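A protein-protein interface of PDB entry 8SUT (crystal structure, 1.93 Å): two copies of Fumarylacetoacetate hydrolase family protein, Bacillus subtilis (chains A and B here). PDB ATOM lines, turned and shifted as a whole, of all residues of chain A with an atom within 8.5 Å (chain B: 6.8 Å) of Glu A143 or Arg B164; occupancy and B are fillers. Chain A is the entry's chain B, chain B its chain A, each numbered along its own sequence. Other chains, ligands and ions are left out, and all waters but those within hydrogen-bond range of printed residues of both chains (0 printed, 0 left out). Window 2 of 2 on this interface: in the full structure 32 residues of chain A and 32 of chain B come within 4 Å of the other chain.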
ATOM      1  N   LYS A 139      14.727  -7.634 -32.657  1.00  0.00           N
ATOM      2  CA  LYS A 139      15.422  -8.825 -33.108  1.00  0.00           C
ATOM      3  C   LYS A 139      14.619  -9.509 -34.216  1.00  0.00           C
ATOM      4  O   LYS A 139      13.392  -9.580 -34.137  1.00  0.00           O
ATOM      5  CB  LYS A 139      15.647  -9.780 -31.944  1.00  0.00           C
ATOM      6  CG  LYS A 139      16.577  -9.236 -30.883  1.00  0.00           C
ATOM      7  CD  LYS A 139      16.749 -10.176 -29.718  1.00  0.00           C
ATOM      8  CE  LYS A 139      17.749  -9.635 -28.731  1.00  0.00           C
ATOM      9  NZ  LYS A 139      17.917 -10.540 -27.563  1.00  0.00           N
ATOM     10  N   SER A 140      15.319  -9.986 -35.257  1.00  0.00           N
ATOM     11  CA  SER A 140      14.668 -10.657 -36.373  1.00  0.00           C
ATOM     12  C   SER A 140      14.289 -12.098 -36.025  1.00  0.00           C
ATOM     13  O   SER A 140      13.402 -12.661 -36.646  1.00  0.00           O
ATOM     14  CB  SER A 140      15.550 -10.615 -37.619  1.00  0.00           C
ATOM     15  OG  SER A 140      16.873 -11.024 -37.319  1.00  0.00           O
ATOM     16  N   HIS A 141      14.960 -12.677 -35.021  1.00  0.00           N
ATOM     17  CA  HIS A 141      14.663 -14.017 -34.527  1.00  0.00           C
ATOM     18  C   HIS A 141      14.722 -15.053 -35.658  1.00  0.00           C
ATOM     19  O   HIS A 141      13.915 -15.985 -35.687  1.00  0.00           O
ATOM     20  CB  HIS A 141      13.314 -14.032 -33.786  1.00  0.00           C
ATOM     21  CG  HIS A 141      13.347 -13.343 -32.467  1.00  0.00           C
ATOM     22  ND1 HIS A 141      14.049 -13.842 -31.389  1.00  0.00           N
ATOM     23  CD2 HIS A 141      12.771 -12.201 -32.055  1.00  0.00           C
ATOM     24  CE1 HIS A 141      13.888 -13.031 -30.353  1.00  0.00           C
ATOM     25  NE2 HIS A 141      13.123 -12.022 -30.738  1.00  0.00           N
ATOM     26  N   GLU A 142      15.714 -14.916 -36.553  1.00  0.00           N
ATOM     27  CA  GLU A 142      15.765 -15.666 -37.800  1.00  0.00           C
ATOM     28  C   GLU A 142      15.920 -17.177 -37.578  1.00  0.00           C
ATOM     29  O   GLU A 142      15.404 -17.964 -38.356  1.00  0.00           O
ATOM     30  CB  GLU A 142      16.879 -15.093 -38.733  1.00  0.00           C
ATOM     31  CG  GLU A 142      18.306 -15.271 -38.228  1.00  0.00           C
ATOM     32  CD  GLU A 142      18.736 -14.528 -36.965  1.00  0.00           C
ATOM     33  OE1 GLU A 142      18.051 -13.569 -36.529  1.00  0.00           O
ATOM     34  OE2 GLU A 142      19.771 -14.939 -36.392  1.00  0.00           O
ATOM     35  N   GLU A 143      16.582 -17.577 -36.489  1.00  0.00           N
ATOM     36  CA  GLU A 143      16.724 -18.980 -36.125  1.00  0.00           C
ATOM     37  C   GLU A 143      15.472 -19.595 -35.492  1.00  0.00           C
ATOM     38  O   GLU A 143      15.457 -20.789 -35.211  1.00  0.00           O
ATOM     39  CB  GLU A 143      17.906 -19.164 -35.149  1.00  0.00           C
ATOM     40  CG  GLU A 143      19.258 -18.792 -35.723  1.00  0.00           C
ATOM     41  CD  GLU A 143      20.419 -19.137 -34.810  1.00  0.00           C
ATOM     42  OE1 GLU A 143      20.514 -18.547 -33.709  1.00  0.00           O
ATOM     43  OE2 GLU A 143      21.228 -20.012 -35.191  1.00  0.00           O
ATOM     44  N   VAL A 144      14.427 -18.783 -35.281  1.00  0.00           N
ATOM     45  CA  VAL A 144      13.184 -19.247 -34.690  1.00  0.00           C
ATOM     46  C   VAL A 144      12.008 -19.168 -35.659  1.00  0.00           C
ATOM     47  O   VAL A 144      11.105 -19.992 -35.598  1.00  0.00           O
ATOM     48  CB  VAL A 144      12.877 -18.423 -33.401  1.00  0.00           C
ATOM     49  CG1 VAL A 144      11.652 -18.963 -32.676  1.00  0.00           C
ATOM     50  CG2 VAL A 144      14.084 -18.379 -32.469  1.00  0.00           C
ATOM     51  N   THR A 145      11.998 -18.142 -36.513  1.00  0.00           N
ATOM     52  CA  THR A 145      10.861 -17.865 -37.375  1.00  0.00           C
ATOM     53  C   THR A 145      11.355 -17.134 -38.615  1.00  0.00           C
ATOM     54  O   THR A 145      12.345 -16.404 -38.551  1.00  0.00           O
ATOM     55  CB  THR A 145       9.768 -17.014 -36.661  1.00  0.00           C
ATOM     56  OG1 THR A 145       8.625 -16.835 -37.518  1.00  0.00           O
ATOM     57  CG2 THR A 145      10.245 -15.630 -36.262  1.00  0.00           C
ATOM     58  N   SER A 146      10.631 -17.332 -39.721  1.00  0.00           N
ATOM     59  CA  SER A 146      10.784 -16.531 -40.927  1.00  0.00           C
ATOM     60  C   SER A 146       9.482 -15.818 -41.263  1.00  0.00           C
ATOM     61  O   SER A 146       9.333 -15.290 -42.361  1.00  0.00           O
ATOM     62  CB  SER A 146      11.226 -17.400 -42.104  1.00  0.00           C
ATOM     63  OG  SER A 146      12.565 -17.832 -41.929  1.00  0.00           O
ATOM     64  N   ASP A 187       4.051 -18.270 -37.875  1.00  0.00           N
ATOM     65  CA  ASP A 187       4.206 -19.717 -37.855  1.00  0.00           C
ATOM     66  C   ASP A 187       4.115 -20.254 -36.426  1.00  0.00           C
ATOM     67  O   ASP A 187       3.466 -21.269 -36.205  1.00  0.00           O
ATOM     68  CB  ASP A 187       5.518 -20.162 -38.531  1.00  0.00           C
ATOM     69  CG  ASP A 187       6.761 -19.389 -38.118  1.00  0.00           C
ATOM     70  OD1 ASP A 187       6.618 -18.372 -37.384  1.00  0.00           O
ATOM     71  OD2 ASP A 187       7.873 -19.780 -38.543  1.00  0.00           O
ATOM     72  N   LEU A 188       4.736 -19.546 -35.468  1.00  0.00           N
ATOM     73  CA  LEU A 188       4.683 -19.921 -34.064  1.00  0.00           C
ATOM     74  C   LEU A 188       3.267 -19.825 -33.508  1.00  0.00           C
ATOM     75  O   LEU A 188       2.884 -20.650 -32.689  1.00  0.00           O
ATOM     76  CB  LEU A 188       5.634 -19.061 -33.205  1.00  0.00           C
ATOM     77  CG  LEU A 188       7.125 -19.246 -33.470  1.00  0.00           C
ATOM     78  CD1 LEU A 188       7.979 -18.542 -32.385  1.00  0.00           C
ATOM     79  CD2 LEU A 188       7.492 -20.729 -33.577  1.00  0.00           C
ATOM     80  N   ARG A 191       1.712 -23.051 -34.828  1.00  0.00           N
ATOM     81  CA  ARG A 191       2.314 -24.211 -34.200  1.00  0.00           C
ATOM     82  C   ARG A 191       1.798 -24.484 -32.783  1.00  0.00           C
ATOM     83  O   ARG A 191       1.551 -25.633 -32.446  1.00  0.00           O
ATOM     84  CB  ARG A 191       3.802 -24.035 -34.183  1.00  0.00           C
ATOM     85  CG  ARG A 191       4.570 -25.233 -33.620  1.00  0.00           C
ATOM     86  CD  ARG A 191       6.064 -24.942 -33.564  1.00  0.00           C
ATOM     87  NE  ARG A 191       6.576 -24.678 -34.903  1.00  0.00           N
ATOM     88  CZ  ARG A 191       7.682 -23.998 -35.168  1.00  0.00           C
ATOM     89  NH1 ARG A 191       8.543 -23.675 -34.215  1.00  0.00           N
ATOM     90  NH2 ARG A 191       7.925 -23.626 -36.422  1.00  0.00           N
ATOM     91  N   ASP A 202      11.369 -11.897 -27.482  1.00  0.00           N
ATOM     92  CA  ASP A 202      12.095 -10.723 -27.002  1.00  0.00           C
ATOM     93  C   ASP A 202      12.091  -9.582 -28.008  1.00  0.00           C
ATOM     94  O   ASP A 202      12.258  -9.809 -29.196  1.00  0.00           O
ATOM     95  CB  ASP A 202      13.562 -11.062 -26.635  1.00  0.00           C
ATOM     96  CG  ASP A 202      13.758 -11.898 -25.368  1.00  0.00           C
ATOM     97  OD1 ASP A 202      12.764 -12.107 -24.625  1.00  0.00           O
ATOM     98  OD2 ASP A 202      14.894 -12.367 -25.131  1.00  0.00           O
ATOM     99  N   GLU A 306      20.823 -10.498 -38.495  1.00  0.00           N
ATOM    100  CA  GLU A 306      20.821 -11.910 -38.171  1.00  0.00           C
ATOM    101  C   GLU A 306      22.024 -12.284 -37.210  1.00  0.00           C
ATOM    102  O   GLU A 306      22.944 -11.487 -37.022  1.00  0.00           O
ATOM    103  CB  GLU A 306      20.807 -12.715 -39.503  1.00  0.00           C
ATOM    104  CG  GLU A 306      22.093 -12.685 -40.339  1.00  0.00           C
ATOM    105  CD  GLU A 306      22.509 -11.415 -41.088  1.00  0.00           C
ATOM    106  OE1 GLU A 306      21.788 -10.381 -41.066  1.00  0.00           O
ATOM    107  OE2 GLU A 306      23.597 -11.476 -41.711  1.00  0.00           O
ATOM    108  N   GLY B 162      17.930 -16.764 -18.669  1.00  0.00           N
ATOM    109  CA  GLY B 162      18.492 -17.395 -19.845  1.00  0.00           C
ATOM    110  C   GLY B 162      17.553 -17.313 -21.035  1.00  0.00           C
ATOM    111  O   GLY B 162      16.335 -17.283 -20.865  1.00  0.00           O
ATOM    112  N   THR B 163      18.150 -17.258 -22.229  1.00  0.00           N
ATOM    113  CA  THR B 163      17.440 -17.501 -23.472  1.00  0.00           C
ATOM    114  C   THR B 163      18.214 -18.575 -24.241  1.00  0.00           C
ATOM    115  O   THR B 163      19.374 -18.838 -23.924  1.00  0.00           O
ATOM    116  CB  THR B 163      17.220 -16.190 -24.222  1.00  0.00           C
ATOM    117  OG1 THR B 163      16.328 -16.474 -25.309  1.00  0.00           O
ATOM    118  CG2 THR B 163      18.534 -15.542 -24.742  1.00  0.00           C
ATOM    119  N   ARG B 164      17.550 -19.218 -25.219  1.00  0.00           N
ATOM    120  CA  ARG B 164      18.161 -20.269 -26.023  1.00  0.00           C
ATOM    121  C   ARG B 164      18.820 -21.294 -25.105  1.00  0.00           C
ATOM    122  O   ARG B 164      19.970 -21.671 -25.290  1.00  0.00           O
ATOM    123  CB  ARG B 164      19.203 -19.706 -27.036  1.00  0.00           C
ATOM    124  CG  ARG B 164      18.628 -18.804 -28.111  1.00  0.00           C
ATOM    125  CD  ARG B 164      17.766 -19.573 -29.081  1.00  0.00           C
ATOM    126  NE  ARG B 164      18.520 -20.602 -29.787  1.00  0.00           N
ATOM    127  CZ  ARG B 164      19.007 -20.467 -31.012  1.00  0.00           C
ATOM    128  NH1 ARG B 164      18.690 -19.429 -31.774  1.00  0.00           N
ATOM    129  NH2 ARG B 164      19.824 -21.402 -31.493  1.00  0.00           N
ATOM    130  N   ILE B 165      18.065 -21.735 -24.099  1.00  0.00           N
ATOM    131  CA  ILE B 165      18.528 -22.755 -23.176  1.00  0.00           C
ATOM    132  C   ILE B 165      18.325 -24.104 -23.863  1.00  0.00           C
ATOM    133  O   ILE B 165      17.248 -24.383 -24.388  1.00  0.00           O
ATOM    134  CB  ILE B 165      17.748 -22.657 -21.843  1.00  0.00           C
ATOM    135  CG1 ILE B 165      17.856 -21.236 -21.214  1.00  0.00           C
ATOM    136  CG2 ILE B 165      18.207 -23.735 -20.881  1.00  0.00           C
ATOM    137  CD1 ILE B 165      16.820 -20.962 -20.121  1.00  0.00           C
ATOM    138  N   SER B 166      19.368 -24.932 -23.860  1.00  0.00           N
ATOM    139  CA  SER B 166      19.264 -26.278 -24.387  1.00  0.00           C
ATOM    140  C   SER B 166      18.591 -27.185 -23.359  1.00  0.00           C
ATOM    141  O   SER B 166      18.658 -26.918 -22.161  1.00  0.00           O
ATOM    142  CB  SER B 166      20.654 -26.803 -24.731  1.00  0.00           C
ATOM    143  OG  SER B 166      21.382 -27.026 -23.533  1.00  0.00           O
ATOM    144  N   ASP B 169      20.896 -28.226 -20.476  1.00  0.00           N
ATOM    145  CA  ASP B 169      21.183 -27.220 -19.458  1.00  0.00           C
ATOM    146  C   ASP B 169      19.970 -26.742 -18.662  1.00  0.00           C
ATOM    147  O   ASP B 169      20.112 -25.878 -17.802  1.00  0.00           O
ATOM    148  CB  ASP B 169      21.810 -25.979 -20.123  1.00  0.00           C
ATOM    149  CG  ASP B 169      23.155 -26.258 -20.764  1.00  0.00           C
ATOM    150  OD1 ASP B 169      23.953 -27.004 -20.151  1.00  0.00           O
ATOM    151  OD2 ASP B 169      23.417 -25.713 -21.866  1.00  0.00           O
ATOM    152  N   ILE B 250      11.321 -25.900 -21.155  1.00  0.00           N
ATOM    153  CA  ILE B 250      12.245 -24.792 -20.985  1.00  0.00           C
ATOM    154  C   ILE B 250      12.962 -24.457 -22.289  1.00  0.00           C
ATOM    155  O   ILE B 250      13.132 -23.282 -22.605  1.00  0.00           O
ATOM    156  CB  ILE B 250      13.200 -25.086 -19.830  1.00  0.00           C
ATOM    157  CG1 ILE B 250      12.419 -25.004 -18.491  1.00  0.00           C
ATOM    158  CG2 ILE B 250      14.427 -24.161 -19.845  1.00  0.00           C
ATOM    159  CD1 ILE B 250      13.193 -25.459 -17.298  1.00  0.00           C
ATOM    160  N   GLU B 251      13.376 -25.490 -23.038  1.00  0.00           N
ATOM    161  CA  GLU B 251      14.039 -25.278 -24.317  1.00  0.00           C
ATOM    162  C   GLU B 251      13.108 -24.589 -25.310  1.00  0.00           C
ATOM    163  O   GLU B 251      13.491 -23.620 -25.959  1.00  0.00           O
ATOM    164  CB  GLU B 251      14.517 -26.616 -24.923  1.00  0.00           C
ATOM    165  CG  GLU B 251      15.222 -26.487 -26.271  1.00  0.00           C
ATOM    166  CD  GLU B 251      15.688 -27.808 -26.867  1.00  0.00           C
ATOM    167  OE1 GLU B 251      14.806 -28.576 -27.314  1.00  0.00           O
ATOM    168  OE2 GLU B 251      16.914 -28.084 -26.886  1.00  0.00           O
ATOM    169  N   LEU B 253      10.275 -22.821 -24.647  1.00  0.00           N
ATOM    170  CA  LEU B 253       9.859 -21.502 -24.193  1.00  0.00           C
ATOM    171  C   LEU B 253      10.948 -20.455 -24.437  1.00  0.00           C
ATOM    172  O   LEU B 253      10.635 -19.331 -24.813  1.00  0.00           O
ATOM    173  CB  LEU B 253       9.525 -21.542 -22.712  1.00  0.00           C
ATOM    174  CG  LEU B 253       8.234 -22.279 -22.368  1.00  0.00           C
ATOM    175  CD1 LEU B 253       8.108 -22.464 -20.899  1.00  0.00           C
ATOM    176  CD2 LEU B 253       7.018 -21.538 -22.899  1.00  0.00           C
ATOM    177  N   SER B 254      12.217 -20.856 -24.248  1.00  0.00           N
ATOM    178  CA  SER B 254      13.330 -19.915 -24.291  1.00  0.00           C
ATOM    179  C   SER B 254      13.931 -19.721 -25.681  1.00  0.00           C
ATOM    180  O   SER B 254      14.838 -18.920 -25.825  1.00  0.00           O
ATOM    181  CB  SER B 254      14.426 -20.332 -23.326  1.00  0.00           C
ATOM    182  OG  SER B 254      15.051 -21.559 -23.686  1.00  0.00           O
ATOM    183  N   LYS B 255      13.423 -20.427 -26.697  1.00  0.00           N
ATOM    184  CA  LYS B 255      13.981 -20.310 -28.037  1.00  0.00           C
ATOM    185  C   LYS B 255      14.117 -18.862 -28.503  1.00  0.00           C
ATOM    186  O   LYS B 255      15.164 -18.496 -29.028  1.00  0.00           O
ATOM    187  CB  LYS B 255      13.183 -21.102 -29.072  1.00  0.00           C
ATOM    188  CG  LYS B 255      13.733 -22.493 -29.307  1.00  0.00           C
ATOM    189  CD  LYS B 255      12.831 -23.371 -30.173  1.00  0.00           C
ATOM    190  CE  LYS B 255      13.388 -24.778 -30.268  1.00  0.00           C
ATOM    191  NZ  LYS B 255      12.403 -25.718 -30.846  1.00  0.00           N
ATOM    192  N   GLY B 256      13.068 -18.052 -28.319  1.00  0.00           N
ATOM    193  CA  GLY B 256      13.131 -16.639 -28.667  1.00  0.00           C
ATOM    194  C   GLY B 256      12.757 -15.661 -27.552  1.00  0.00           C
ATOM    195  O   GLY B 256      12.422 -14.511 -27.829  1.00  0.00           O
ATOM    196  N   MET B 257      12.837 -16.123 -26.301  1.00  0.00           N
ATOM    197  CA  MET B 257      12.303 -15.395 -25.164  1.00  0.00           C
ATOM    198  C   MET B 257      13.203 -15.655 -23.951  1.00  0.00           C
ATOM    199  O   MET B 257      13.681 -16.769 -23.741  1.00  0.00           O
ATOM    200  CB  MET B 257      10.857 -15.859 -24.928  1.00  0.00           C
ATOM    201  CG  MET B 257      10.198 -15.262 -23.728  1.00  0.00           C
ATOM    202  SD  MET B 257       8.454 -15.728 -23.615  1.00  0.00           S
ATOM    203  CE  MET B 257       8.584 -17.284 -22.728  1.00  0.00           C
ATOM    204  N   THR B 258      13.464 -14.604 -23.173  1.00  0.00           N
ATOM    205  CA  THR B 258      14.290 -14.718 -21.988  1.00  0.00           C
ATOM    206  C   THR B 258      13.391 -15.187 -20.850  1.00  0.00           C
ATOM    207  O   THR B 258      12.325 -14.623 -20.627  1.00  0.00           O
ATOM    208  CB  THR B 258      14.995 -13.383 -21.713  1.00  0.00           C
ATOM    209  OG1 THR B 258      15.852 -13.109 -22.825  1.00  0.00           O
ATOM    210  CG2 THR B 258      15.804 -13.412 -20.439  1.00  0.00           C
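OD2 of Asp A202 is in hydrogen-bond range of OG1 of Thr B258, at 2.6 Å. The backbone NH of Asp A202 sits at hydrogen-bond distance from the backbone carbonyl oxygen of Gly B256 (2.8 Å). The guanidinium group (NH1) of Arg B164 is in salt-bridge range of the side-chain carboxylate (OE1) of Glu A143 (2.8 Å).
The backbone NH (N) of Arg B164 is in hydrogen-bond range of the backbone carbonyl oxygen (O) of Ser B254. NE2 of His A141 lies within hydrogen-bond range of O of Asp A202, at 2.8 Å. OG1 of Thr B163 sits at hydrogen-bond distance from O of Met B257, 3.1 Å away.
Among the printed residues, merely in contact across the chains: His A141 with Gly B256, Val A144 with Lys B255 and Asp A202 with Met B257.
Glu A143 touches just one residue of chain B: Arg B164 (2.8 Å). Arg B164 touches just one residue of chain A: Glu A143 (2.8 Å). No residue of chain A comes within 4 Å of Thr B163. Printed residues of chain A within 4 Å of Lys B255: Val A144 (3.6 Å). Of the printed residues of chain A, Met B257 touches Asp A202. Of the printed residues of chain A, Thr B258 touches Asp A202 (2.6 Å). Printed residues of chain A within 4 Å of Gly B256: His A141 (3.3 Å) and Asp A202 (2.8 Å). Of the printed residues of chain B, Val A144 touches Lys B255. Glu B251 touches none of the printed residues of chain A. The nearest residue of chain A that does not touch Arg B164 is Val A144 (4.8 Å).
Of the 13 printed residues of chain A, 4 touch a printed residue of chain B. Of the 14 printed residues of chain B, 5 touch a printed residue of chain A. Among the printed residues, 6 pairs touch across the chains.
No position is printed for both chains. Of the 6 pairs that touch across the chains among the printed residues, none has its exchanged pair printed and touching as well.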
